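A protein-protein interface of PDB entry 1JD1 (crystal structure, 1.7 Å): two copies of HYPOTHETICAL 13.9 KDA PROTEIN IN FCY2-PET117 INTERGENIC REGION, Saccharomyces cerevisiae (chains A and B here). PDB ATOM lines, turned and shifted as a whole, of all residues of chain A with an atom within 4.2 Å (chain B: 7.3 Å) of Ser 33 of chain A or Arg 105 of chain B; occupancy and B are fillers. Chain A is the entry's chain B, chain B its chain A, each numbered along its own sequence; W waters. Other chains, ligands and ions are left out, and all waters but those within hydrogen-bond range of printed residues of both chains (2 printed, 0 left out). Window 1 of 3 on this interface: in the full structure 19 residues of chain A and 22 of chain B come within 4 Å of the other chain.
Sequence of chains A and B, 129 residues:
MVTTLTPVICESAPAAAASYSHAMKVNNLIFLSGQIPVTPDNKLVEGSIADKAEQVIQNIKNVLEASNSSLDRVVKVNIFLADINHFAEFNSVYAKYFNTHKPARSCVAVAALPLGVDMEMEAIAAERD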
ATOM      1  N   ALA A  18      26.346 -30.020 -35.744  1.00  0.00           N
ATOM      2  CA  ALA A  18      26.921 -28.984 -34.906  1.00  0.00           C
ATOM      3  C   ALA A  18      27.444 -29.682 -33.665  1.00  0.00           C
ATOM      4  O   ALA A  18      27.460 -30.909 -33.612  1.00  0.00           O
ATOM      5  CB  ALA A  18      25.865 -27.937 -34.545  1.00  0.00           C
ATOM      6  N   TYR A  20      26.925 -31.288 -30.763  1.00  0.00           N
ATOM      7  CA  TYR A  20      25.947 -31.949 -29.916  1.00  0.00           C
ATOM      8  C   TYR A  20      26.049 -33.470 -29.986  1.00  0.00           C
ATOM      9  O   TYR A  20      26.526 -34.019 -30.977  1.00  0.00           O
ATOM     10  CB  TYR A  20      24.532 -31.493 -30.321  1.00  0.00           C
ATOM     11  CG  TYR A  20      24.099 -31.758 -31.765  1.00  0.00           C
ATOM     12  CD1 TYR A  20      23.552 -32.998 -32.144  1.00  0.00           C
ATOM     13  CD2 TYR A  20      24.153 -30.750 -32.731  1.00  0.00           C
ATOM     14  CE1 TYR A  20      23.069 -33.218 -33.442  1.00  0.00           C
ATOM     15  CE2 TYR A  20      23.669 -30.958 -34.049  1.00  0.00           C
ATOM     16  CZ  TYR A  20      23.132 -32.203 -34.388  1.00  0.00           C
ATOM     17  OH  TYR A  20      22.706 -32.436 -35.680  1.00  0.00           O
ATOM     18  N   SER A  21      25.605 -34.139 -28.923  1.00  0.00           N
ATOM     19  CA  SER A  21      25.584 -35.596 -28.864  1.00  0.00           C
ATOM     20  C   SER A  21      24.242 -36.031 -29.465  1.00  0.00           C
ATOM     21  O   SER A  21      23.328 -35.212 -29.559  1.00  0.00           O
ATOM     22  CB  SER A  21      25.660 -36.066 -27.418  1.00  0.00           C
ATOM     23  OG  SER A  21      26.869 -35.625 -26.811  1.00  0.00           O
ATOM     24  N   HIS A  22      24.114 -37.287 -29.884  1.00  0.00           N
ATOM     25  CA  HIS A  22      22.834 -37.727 -30.437  1.00  0.00           C
ATOM     26  C   HIS A  22      21.766 -37.720 -29.336  1.00  0.00           C
ATOM     27  O   HIS A  22      20.592 -37.478 -29.606  1.00  0.00           O
ATOM     28  CB  HIS A  22      22.941 -39.128 -31.050  1.00  0.00           C
ATOM     29  CG  HIS A  22      23.814 -39.191 -32.262  1.00  0.00           C
ATOM     30  ND1 HIS A  22      23.572 -38.452 -33.401  1.00  0.00           N
ATOM     31  CD2 HIS A  22      24.939 -39.899 -32.508  1.00  0.00           C
ATOM     32  CE1 HIS A  22      24.511 -38.704 -34.295  1.00  0.00           C
ATOM     33  NE2 HIS A  22      25.353 -39.580 -33.777  1.00  0.00           N
ATOM     34  N   PHE A  31      17.328 -37.509 -23.285  1.00  0.00           N
ATOM     35  CA  PHE A  31      16.909 -36.412 -24.149  1.00  0.00           C
ATOM     36  C   PHE A  31      17.607 -36.610 -25.505  1.00  0.00           C
ATOM     37  O   PHE A  31      18.847 -36.567 -25.610  1.00  0.00           O
ATOM     38  CB  PHE A  31      17.285 -35.050 -23.533  1.00  0.00           C
ATOM     39  CG  PHE A  31      16.451 -34.677 -22.336  1.00  0.00           C
ATOM     40  CD1 PHE A  31      16.668 -35.290 -21.099  1.00  0.00           C
ATOM     41  CD2 PHE A  31      15.393 -33.771 -22.460  1.00  0.00           C
ATOM     42  CE1 PHE A  31      15.840 -35.009 -20.009  1.00  0.00           C
ATOM     43  CE2 PHE A  31      14.564 -33.486 -21.373  1.00  0.00           C
ATOM     44  CZ  PHE A  31      14.784 -34.104 -20.153  1.00  0.00           C
ATOM     45  N   LEU A  32      16.803 -36.840 -26.542  1.00  0.00           N
ATOM     46  CA  LEU A  32      17.334 -37.054 -27.880  1.00  0.00           C
ATOM     47  C   LEU A  32      17.384 -35.772 -28.711  1.00  0.00           C
ATOM     48  O   LEU A  32      16.449 -34.946 -28.695  1.00  0.00           O
ATOM     49  CB  LEU A  32      16.490 -38.110 -28.625  1.00  0.00           C
ATOM     50  CG  LEU A  32      16.538 -39.562 -28.124  1.00  0.00           C
ATOM     51  CD1 LEU A  32      15.597 -39.765 -26.928  1.00  0.00           C
ATOM     52  CD2 LEU A  32      16.159 -40.493 -29.278  1.00  0.00           C
ATOM     53  N   SER A  33      18.468 -35.619 -29.463  1.00  0.00           N
ATOM     54  CA  SER A  33      18.633 -34.460 -30.333  1.00  0.00           C
ATOM     55  C   SER A  33      17.690 -34.530 -31.529  1.00  0.00           C
ATOM     56  O   SER A  33      17.203 -35.609 -31.890  1.00  0.00           O
ATOM     57  CB  SER A  33      20.079 -34.382 -30.845  1.00  0.00           C
ATOM     58  OG  SER A  33      20.959 -34.122 -29.761  1.00  0.00           O
ATOM     59  N   GLY A  34      17.388 -33.367 -32.102  1.00  0.00           N
ATOM     60  CA  GLY A  34      16.533 -33.313 -33.269  1.00  0.00           C
ATOM     61  C   GLY A  34      17.138 -34.097 -34.420  1.00  0.00           C
ATOM     62  O   GLY A  34      18.324 -33.968 -34.705  1.00  0.00           O
ATOM     63  N   GLN A  35      16.321 -34.925 -35.064  1.00  0.00           N
ATOM     64  CA  GLN A  35      16.744 -35.737 -36.216  1.00  0.00           C
ATOM     65  C   GLN A  35      16.035 -35.248 -37.471  1.00  0.00           C
ATOM     66  O   GLN A  35      14.841 -34.919 -37.438  1.00  0.00           O
ATOM     67  CB  GLN A  35      16.396 -37.212 -35.992  1.00  0.00           C
ATOM     68  CG  GLN A  35      17.303 -37.915 -35.008  1.00  0.00           C
ATOM     69  CD  GLN A  35      18.736 -38.013 -35.519  1.00  0.00           C
ATOM     70  OE1 GLN A  35      19.690 -37.902 -34.747  1.00  0.00           O
ATOM     71  NE2 GLN A  35      18.890 -38.209 -36.820  1.00  0.00           N
ATOM     72  N   MET A 121      12.512 -34.027 -35.861  1.00  0.00           N
ATOM     73  CA  MET A 121      11.829 -34.660 -34.743  1.00  0.00           C
ATOM     74  C   MET A 121      12.807 -34.888 -33.598  1.00  0.00           C
ATOM     75  O   MET A 121      13.924 -35.370 -33.830  1.00  0.00           O
ATOM     76  CB  MET A 121      11.263 -36.013 -35.206  1.00  0.00           C
ATOM     77  CG  MET A 121      10.686 -36.917 -34.108  1.00  0.00           C
ATOM     78  SD  MET A 121       9.938 -38.497 -34.741  1.00  0.00           S
ATOM     79  CE  MET A 121       9.950 -39.312 -33.465  1.00  0.00           C
ATOM     80  N   GLU A 122      12.412 -34.505 -32.388  1.00  0.00           N
ATOM     81  CA  GLU A 122      13.218 -34.733 -31.198  1.00  0.00           C
ATOM     82  C   GLU A 122      12.335 -35.535 -30.253  1.00  0.00           C
ATOM     83  O   GLU A 122      11.119 -35.631 -30.447  1.00  0.00           O
ATOM     84  CB  GLU A 122      13.662 -33.413 -30.527  1.00  0.00           C
ATOM     85  CG  GLU A 122      12.510 -32.533 -30.089  1.00  0.00           C
ATOM     86  CD  GLU A 122      12.948 -31.322 -29.270  1.00  0.00           C
ATOM     87  OE1 GLU A 122      12.124 -30.838 -28.464  1.00  0.00           O
ATOM     88  OE2 GLU A 122      14.100 -30.855 -29.425  1.00  0.00           O
ATOM     89  N   VAL B  75      21.978 -30.643 -20.076  1.00  0.00           N
ATOM     90  CA  VAL B  75      21.507 -31.892 -20.667  1.00  0.00           C
ATOM     91  C   VAL B  75      21.030 -31.749 -22.118  1.00  0.00           C
ATOM     92  O   VAL B  75      21.445 -32.497 -23.000  1.00  0.00           O
ATOM     93  CB  VAL B  75      20.334 -32.468 -19.825  1.00  0.00           C
ATOM     94  CG1 VAL B  75      19.821 -33.752 -20.447  1.00  0.00           C
ATOM     95  CG2 VAL B  75      20.804 -32.725 -18.384  1.00  0.00           C
ATOM     96  N   LYS B  76      20.164 -30.768 -22.345  1.00  0.00           N
ATOM     97  CA  LYS B  76      19.537 -30.537 -23.641  1.00  0.00           C
ATOM     98  C   LYS B  76      19.392 -29.046 -23.878  1.00  0.00           C
ATOM     99  O   LYS B  76      19.084 -28.294 -22.955  1.00  0.00           O
ATOM    100  CB  LYS B  76      18.130 -31.178 -23.633  1.00  0.00           C
ATOM    101  CG  LYS B  76      17.242 -30.824 -24.803  1.00  0.00           C
ATOM    102  CD  LYS B  76      17.703 -31.505 -26.105  1.00  0.00           C
ATOM    103  CE  LYS B  76      16.866 -31.025 -27.299  1.00  0.00           C
ATOM    104  NZ  LYS B  76      15.414 -31.299 -27.040  1.00  0.00           N
ATOM    105  N   VAL B  77      19.619 -28.633 -25.116  1.00  0.00           N
ATOM    106  CA  VAL B  77      19.499 -27.241 -25.521  1.00  0.00           C
ATOM    107  C   VAL B  77      18.602 -27.174 -26.740  1.00  0.00           C
ATOM    108  O   VAL B  77      18.683 -28.022 -27.624  1.00  0.00           O
ATOM    109  CB  VAL B  77      20.863 -26.650 -25.924  1.00  0.00           C
ATOM    110  CG1 VAL B  77      20.668 -25.297 -26.565  1.00  0.00           C
ATOM    111  CG2 VAL B  77      21.769 -26.574 -24.712  1.00  0.00           C
ATOM    112  N   ASN B  78      17.703 -26.195 -26.768  1.00  0.00           N
ATOM    113  CA  ASN B  78      16.862 -25.979 -27.924  1.00  0.00           C
ATOM    114  C   ASN B  78      17.138 -24.579 -28.428  1.00  0.00           C
ATOM    115  O   ASN B  78      17.085 -23.607 -27.653  1.00  0.00           O
ATOM    116  CB  ASN B  78      15.369 -26.110 -27.585  1.00  0.00           C
ATOM    117  CG  ASN B  78      14.913 -27.552 -27.559  1.00  0.00           C
ATOM    118  OD1 ASN B  78      15.209 -28.292 -26.620  1.00  0.00           O
ATOM    119  ND2 ASN B  78      14.200 -27.966 -28.603  1.00  0.00           N
ATOM    120  N   ILE B  79      17.429 -24.476 -29.720  1.00  0.00           N
ATOM    121  CA  ILE B  79      17.701 -23.192 -30.343  1.00  0.00           C
ATOM    122  C   ILE B  79      16.581 -22.821 -31.308  1.00  0.00           C
ATOM    123  O   ILE B  79      16.119 -23.656 -32.097  1.00  0.00           O
ATOM    124  CB  ILE B  79      19.046 -23.219 -31.148  1.00  0.00           C
ATOM    125  CG1 ILE B  79      20.192 -23.660 -30.230  1.00  0.00           C
ATOM    126  CG2 ILE B  79      19.317 -21.857 -31.777  1.00  0.00           C
ATOM    127  CD1 ILE B  79      20.345 -22.825 -28.966  1.00  0.00           C
ATOM    128  N   LEU B  81      15.933 -19.940 -34.170  1.00  0.00           N
ATOM    129  CA  LEU B  81      16.540 -18.845 -34.930  1.00  0.00           C
ATOM    130  C   LEU B  81      15.492 -18.067 -35.696  1.00  0.00           C
ATOM    131  O   LEU B  81      14.521 -18.642 -36.194  1.00  0.00           O
ATOM    132  CB  LEU B  81      17.570 -19.391 -35.926  1.00  0.00           C
ATOM    133  CG  LEU B  81      18.716 -20.236 -35.370  1.00  0.00           C
ATOM    134  CD1 LEU B  81      19.496 -20.854 -36.548  1.00  0.00           C
ATOM    135  CD2 LEU B  81      19.647 -19.379 -34.514  1.00  0.00           C
ATOM    136  N   PHE B  87      22.528 -19.983 -38.799  1.00  0.00           N
ATOM    137  CA  PHE B  87      22.923 -21.281 -38.248  1.00  0.00           C
ATOM    138  C   PHE B  87      24.445 -21.411 -38.054  1.00  0.00           C
ATOM    139  O   PHE B  87      24.930 -21.600 -36.940  1.00  0.00           O
ATOM    140  CB  PHE B  87      22.395 -22.392 -39.186  1.00  0.00           C
ATOM    141  CG  PHE B  87      22.537 -23.795 -38.648  1.00  0.00           C
ATOM    142  CD1 PHE B  87      21.900 -24.183 -37.470  1.00  0.00           C
ATOM    143  CD2 PHE B  87      23.250 -24.749 -39.366  1.00  0.00           C
ATOM    144  CE1 PHE B  87      21.966 -25.507 -37.019  1.00  0.00           C
ATOM    145  CE2 PHE B  87      23.324 -26.070 -38.926  1.00  0.00           C
ATOM    146  CZ  PHE B  87      22.678 -26.445 -37.749  1.00  0.00           C
ATOM    147  N   PHE B  90      25.989 -18.871 -35.540  1.00  0.00           N
ATOM    148  CA  PHE B  90      25.600 -19.202 -34.180  1.00  0.00           C
ATOM    149  C   PHE B  90      26.383 -20.429 -33.733  1.00  0.00           C
ATOM    150  O   PHE B  90      26.961 -20.438 -32.649  1.00  0.00           O
ATOM    151  CB  PHE B  90      24.102 -19.502 -34.088  1.00  0.00           C
ATOM    152  CG  PHE B  90      23.663 -19.916 -32.708  1.00  0.00           C
ATOM    153  CD1 PHE B  90      23.371 -18.957 -31.743  1.00  0.00           C
ATOM    154  CD2 PHE B  90      23.637 -21.261 -32.352  1.00  0.00           C
ATOM    155  CE1 PHE B  90      23.070 -19.332 -30.446  1.00  0.00           C
ATOM    156  CE2 PHE B  90      23.340 -21.656 -31.059  1.00  0.00           C
ATOM    157  CZ  PHE B  90      23.056 -20.688 -30.093  1.00  0.00           C
ATOM    158  N   ASN B  91      26.407 -21.466 -34.568  1.00  0.00           N
ATOM    159  CA  ASN B  91      27.119 -22.689 -34.213  1.00  0.00           C
ATOM    160  C   ASN B  91      28.571 -22.467 -33.832  1.00  0.00           C
ATOM    161  O   ASN B  91      29.085 -23.139 -32.945  1.00  0.00           O
ATOM    162  CB  ASN B  91      27.061 -23.721 -35.349  1.00  0.00           C
ATOM    163  CG  ASN B  91      25.702 -24.372 -35.470  1.00  0.00           C
ATOM    164  OD1 ASN B  91      24.917 -24.371 -34.510  1.00  0.00           O
ATOM    165  ND2 ASN B  91      25.412 -24.944 -36.644  1.00  0.00           N
ATOM    166  N   SER B  92      29.240 -21.543 -34.513  1.00  0.00           N
ATOM    167  CA  SER B  92      30.643 -21.274 -34.222  1.00  0.00           C
ATOM    168  C   SER B  92      30.836 -20.786 -32.779  1.00  0.00           C
ATOM    169  O   SER B  92      31.741 -21.233 -32.083  1.00  0.00           O
ATOM    170  CB  SER B  92      31.191 -20.257 -35.226  1.00  0.00           C
ATOM    171  OG  SER B  92      32.579 -20.069 -35.032  1.00  0.00           O
ATOM    172  N   TYR B  94      28.565 -21.177 -30.310  1.00  0.00           N
ATOM    173  CA  TYR B  94      28.054 -22.274 -29.500  1.00  0.00           C
ATOM    174  C   TYR B  94      29.157 -23.295 -29.176  1.00  0.00           C
ATOM    175  O   TYR B  94      29.300 -23.729 -28.032  1.00  0.00           O
ATOM    176  CB  TYR B  94      26.921 -22.975 -30.266  1.00  0.00           C
ATOM    177  CG  TYR B  94      26.172 -24.015 -29.455  1.00  0.00           C
ATOM    178  CD1 TYR B  94      25.176 -23.630 -28.558  1.00  0.00           C
ATOM    179  CD2 TYR B  94      26.444 -25.378 -29.602  1.00  0.00           C
ATOM    180  CE1 TYR B  94      24.456 -24.572 -27.829  1.00  0.00           C
ATOM    181  CE2 TYR B  94      25.730 -26.344 -28.876  1.00  0.00           C
ATOM    182  CZ  TYR B  94      24.737 -25.923 -27.995  1.00  0.00           C
ATOM    183  OH  TYR B  94      24.011 -26.840 -27.295  1.00  0.00           O
ATOM    184  N   ALA B  95      29.929 -23.665 -30.198  1.00  0.00           N
ATOM    185  CA  ALA B  95      30.991 -24.663 -30.061  1.00  0.00           C
ATOM    186  C   ALA B  95      32.073 -24.304 -29.052  1.00  0.00           C
ATOM    187  O   ALA B  95      32.760 -25.192 -28.538  1.00  0.00           O
ATOM    188  CB  ALA B  95      31.617 -24.927 -31.418  1.00  0.00           C
ATOM    189  N   PHE B  98      30.432 -25.384 -25.653  1.00  0.00           N
ATOM    190  CA  PHE B  98      30.086 -26.795 -25.596  1.00  0.00           C
ATOM    191  C   PHE B  98      31.059 -27.549 -26.486  1.00  0.00           C
ATOM    192  O   PHE B  98      30.775 -27.844 -27.643  1.00  0.00           O
ATOM    193  CB  PHE B  98      28.636 -27.002 -26.037  1.00  0.00           C
ATOM    194  CG  PHE B  98      27.643 -26.304 -25.147  1.00  0.00           C
ATOM    195  CD1 PHE B  98      27.003 -25.139 -25.568  1.00  0.00           C
ATOM    196  CD2 PHE B  98      27.396 -26.778 -23.858  1.00  0.00           C
ATOM    197  CE1 PHE B  98      26.124 -24.451 -24.709  1.00  0.00           C
ATOM    198  CE2 PHE B  98      26.517 -26.093 -22.991  1.00  0.00           C
ATOM    199  CZ  PHE B  98      25.888 -24.932 -23.424  1.00  0.00           C
ATOM    200  N   LYS B 102      29.029 -31.986 -24.783  1.00  0.00           N
ATOM    201  CA  LYS B 102      28.094 -31.710 -25.859  1.00  0.00           C
ATOM    202  C   LYS B 102      26.673 -32.167 -25.560  1.00  0.00           C
ATOM    203  O   LYS B 102      26.336 -33.341 -25.701  1.00  0.00           O
ATOM    204  CB  LYS B 102      28.594 -32.366 -27.144  1.00  0.00           C
ATOM    205  CG  LYS B 102      29.987 -31.889 -27.511  1.00  0.00           C
ATOM    206  CD  LYS B 102      30.477 -32.455 -28.827  1.00  0.00           C
ATOM    207  CE  LYS B 102      31.853 -31.871 -29.147  1.00  0.00           C
ATOM    208  NZ  LYS B 102      32.428 -32.506 -30.355  1.00  0.00           N
ATOM    209  N   PRO B 103      25.826 -31.229 -25.116  1.00  0.00           N
ATOM    210  CA  PRO B 103      24.420 -31.515 -24.791  1.00  0.00           C
ATOM    211  C   PRO B 103      23.659 -32.016 -26.005  1.00  0.00           C
ATOM    212  O   PRO B 103      24.093 -31.807 -27.136  1.00  0.00           O
ATOM    213  CB  PRO B 103      23.882 -30.153 -24.364  1.00  0.00           C
ATOM    214  CG  PRO B 103      25.077 -29.495 -23.733  1.00  0.00           C
ATOM    215  CD  PRO B 103      26.208 -29.873 -24.689  1.00  0.00           C
ATOM    216  N   ALA B 104      22.523 -32.679 -25.769  1.00  0.00           N
ATOM    217  CA  ALA B 104      21.661 -33.094 -26.871  1.00  0.00           C
ATOM    218  C   ALA B 104      21.182 -31.717 -27.342  1.00  0.00           C
ATOM    219  O   ALA B 104      21.251 -30.758 -26.570  1.00  0.00           O
ATOM    220  CB  ALA B 104      20.489 -33.921 -26.350  1.00  0.00           C
ATOM    221  N   ARG B 105      20.700 -31.600 -28.577  1.00  0.00           N
ATOM    222  CA  ARG B 105      20.275 -30.286 -29.074  1.00  0.00           C
ATOM    223  C   ARG B 105      19.301 -30.360 -30.240  1.00  0.00           C
ATOM    224  O   ARG B 105      19.252 -31.353 -30.970  1.00  0.00           O
ATOM    225  CB  ARG B 105      21.499 -29.497 -29.542  1.00  0.00           C
ATOM    226  CG  ARG B 105      21.295 -27.979 -29.610  1.00  0.00           C
ATOM    227  CD  ARG B 105      22.510 -27.299 -30.257  1.00  0.00           C
ATOM    228  NE  ARG B 105      22.373 -27.287 -31.708  1.00  0.00           N
ATOM    229  CZ  ARG B 105      23.076 -26.499 -32.515  1.00  0.00           C
ATOM    230  NH1 ARG B 105      23.978 -25.663 -32.008  1.00  0.00           N
ATOM    231  NH2 ARG B 105      22.847 -26.517 -33.821  1.00  0.00           N
ATOM    232  N   SER B 106      18.522 -29.294 -30.402  1.00  0.00           N
ATOM    233  CA  SER B 106      17.612 -29.163 -31.528  1.00  0.00           C
ATOM    234  C   SER B 106      17.738 -27.723 -31.956  1.00  0.00           C
ATOM    235  O   SER B 106      18.110 -26.859 -31.145  1.00  0.00           O
ATOM    236  CB  SER B 106      16.159 -29.458 -31.158  1.00  0.00           C
ATOM    237  OG  SER B 106      16.019 -30.854 -30.993  1.00  0.00           O
ATOM    238  N   CYS B 107      17.458 -27.470 -33.230  1.00  0.00           N
ATOM    239  CA  CYS B 107      17.549 -26.124 -33.776  1.00  0.00           C
ATOM    240  C   CYS B 107      16.592 -25.989 -34.954  1.00  0.00           C
ATOM    241  O   CYS B 107      16.570 -26.813 -35.873  1.00  0.00           O
ATOM    242  CB  CYS B 107      18.979 -25.821 -34.226  1.00  0.00           C
ATOM    243  SG  CYS B 107      19.198 -24.140 -34.880  1.00  0.00           S
ATOM    244  N   GLU B 122      16.882 -22.028 -24.998  1.00  0.00           N
ATOM    245  CA  GLU B 122      16.431 -22.578 -23.730  1.00  0.00           C
ATOM    246  C   GLU B 122      17.281 -23.823 -23.478  1.00  0.00           C
ATOM    247  O   GLU B 122      17.980 -24.321 -24.384  1.00  0.00           O
ATOM    248  CB  GLU B 122      14.939 -22.953 -23.775  1.00  0.00           C
ATOM    249  CG  GLU B 122      14.585 -23.920 -24.905  1.00  0.00           C
ATOM    250  CD  GLU B 122      13.179 -24.476 -24.794  1.00  0.00           C
ATOM    251  OE1 GLU B 122      12.250 -23.736 -24.398  1.00  0.00           O
ATOM    252  OE2 GLU B 122      13.003 -25.672 -25.114  1.00  0.00           O
HETATM  253  O   HOH W   1      12.536 -32.661 -26.373  1.00  0.00           O
HETATM  254  O   HOH W   2      29.656 -33.284 -31.980  1.00  0.00           O
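Water W1 lies within hydrogen-bond range of the side-chain carboxylate (OE1) of Glu 122 of chain A (2.8 Å) and the side-chain amino group (NZ) of Lys 76 of chain B (3.3 Å). Water W2 bridges NZ of Lys 102 of chain B and O of Tyr 20 of chain A.
Of the printed residues of chain B, Ala 18 of chain A touches Asn 91 (3.7 Å) and Arg 105 (3.4 Å). Ser 33 of chain A touches just these residues of chain B: Ala 104 (3.1 Å) and Arg 105 (2.8 Å). Of the printed residues of chain A, Val 75 of chain B touches Phe 31 (3.6 Å). Printed residues of chain A within 4 Å of Asn 78 of chain B: Glu 122. Phe 87 of chain B touches none of the printed residues of chain A. Printed residues of chain A within 4 Å of Lys 102 of chain B: Tyr 20 (3.9 Å) and Ser 21 (2.6 Å). Of chain A, only Ala 18 (3.4 Å), Tyr 20 (3.7 Å), Ser 33 (2.8 Å) and Gly 34 (3.0 Å) come within 4 Å of Arg 105 of chain B. Glu 122 of chain B touches none of the printed residues of chain A. The nearest residue of chain B that does not touch Ser 33 of chain A is Ser 106 of chain B (4.1 Å). The nearest printed residue of chain A that does not touch Arg 105 of chain B is Ser 21 of chain A (4.6 Å). The nearest printed residue of chain B that does not touch Gly 34 of chain A is Lys 76 of chain B (5.4 Å).
1 position is printed for both chains.
O of Val 77 of chain B lies within hydrogen-bond range of N of Ser 106 of chain B, 3.1 Å away. The backbone NH of Ser 33 of chain A is in hydrogen-bond range of the backbone carbonyl oxygen of His 22 of chain A. O of Ala 104 of chain B is in hydrogen-bond range of N of Val 77 of chain B (3.0 Å). The backbone carbonyl oxygen (O) of Phe 87 of chain B sits close to the side-chain amide nitrogen (ND2) of Asn 91 of chain B (3.4 Å). The backbone NH (N) of Ile 79 of chain B lies within hydrogen-bond range of the backbone carbonyl oxygen (O) of Ser 106 of chain B, 2.9 Å away. N of Asn 78 of chain B is in hydrogen-bond range of O of Glu 122 of chain B (3.0 Å).
CB of Ala 18 of chain A touches ND2 of Asn 91 of chain B, at 3.7 Å. Ala 18 of chain A touches Arg 105 of chain B (CB to NH2, 3.4 Å). CB of Lys 102 of chain B touches CA of Tyr 20 of chain A, at 3.9 Å. Tyr 20 of chain A touches Pro 103 of chain B. Tyr 20 of chain A touches Arg 105 of chain B (CB to CB, 3.7 Å). O of Ser 21 of chain A touches CA of Ala 104 of chain B (3.8 Å). Val 75 of chain B touches Phe 31 of chain A (CG1 to CD1, 3.6 Å). Lys 76 of chain B touches Phe 31 of chain A. Phe 31 of chain A touches Ala 104 of chain B. Ala 104 of chain B touches Ser 33 of chain A (CA to OG, 3.1 Å).
Hydrophobic or aromatic side chains of chain B within 4 Å of the printed part of chain A: Val 75 and Ala 104. Hydrophobic or aromatic side chains of chain A within 4 Å of the printed part of chain B: Ala 18, Tyr 20 and Phe 31. Among the printed residues, Asp or Glu carboxylates within 4 Å of a Lys or Arg side-chain nitrogen of the other chain: Glu 122 of chain A with Lys 76 of chain B (2.8 Å).
O of Lys 102 of chain B lies within hydrogen-bond range of OG of Ser 21 of chain A. The backbone NH (N) of Gly 34 of chain A sits at hydrogen-bond distance from the side-chain hydroxyl (OG) of Ser 106 of chain B, at 3.1 Å. The side-chain hydroxyl of Ser 106 of chain B sits at hydrogen-bond distance from the side-chain carboxylate of Glu 122 of chain A. The backbone carbonyl oxygen (O) of Arg 105 of chain B sits at hydrogen-bond distance from the backbone NH (N) of Gly 34 of chain A. The side-chain amide nitrogen of Asn 78 of chain B lies within hydrogen-bond range of the side-chain carboxylate of Glu 122 of chain A (3.0 Å). O of Pro 103 of chain B lies within hydrogen-bond range of N of Ser 21 of chain A, at 3.3 Å. OG of Ser 33 of chain A lies within hydrogen-bond range of N of Arg 105 of chain B, 2.8 Å away. NZ of Lys 76 of chain B is in salt-bridge range of OE2 of Glu 122 of chain A (2.8 Å).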
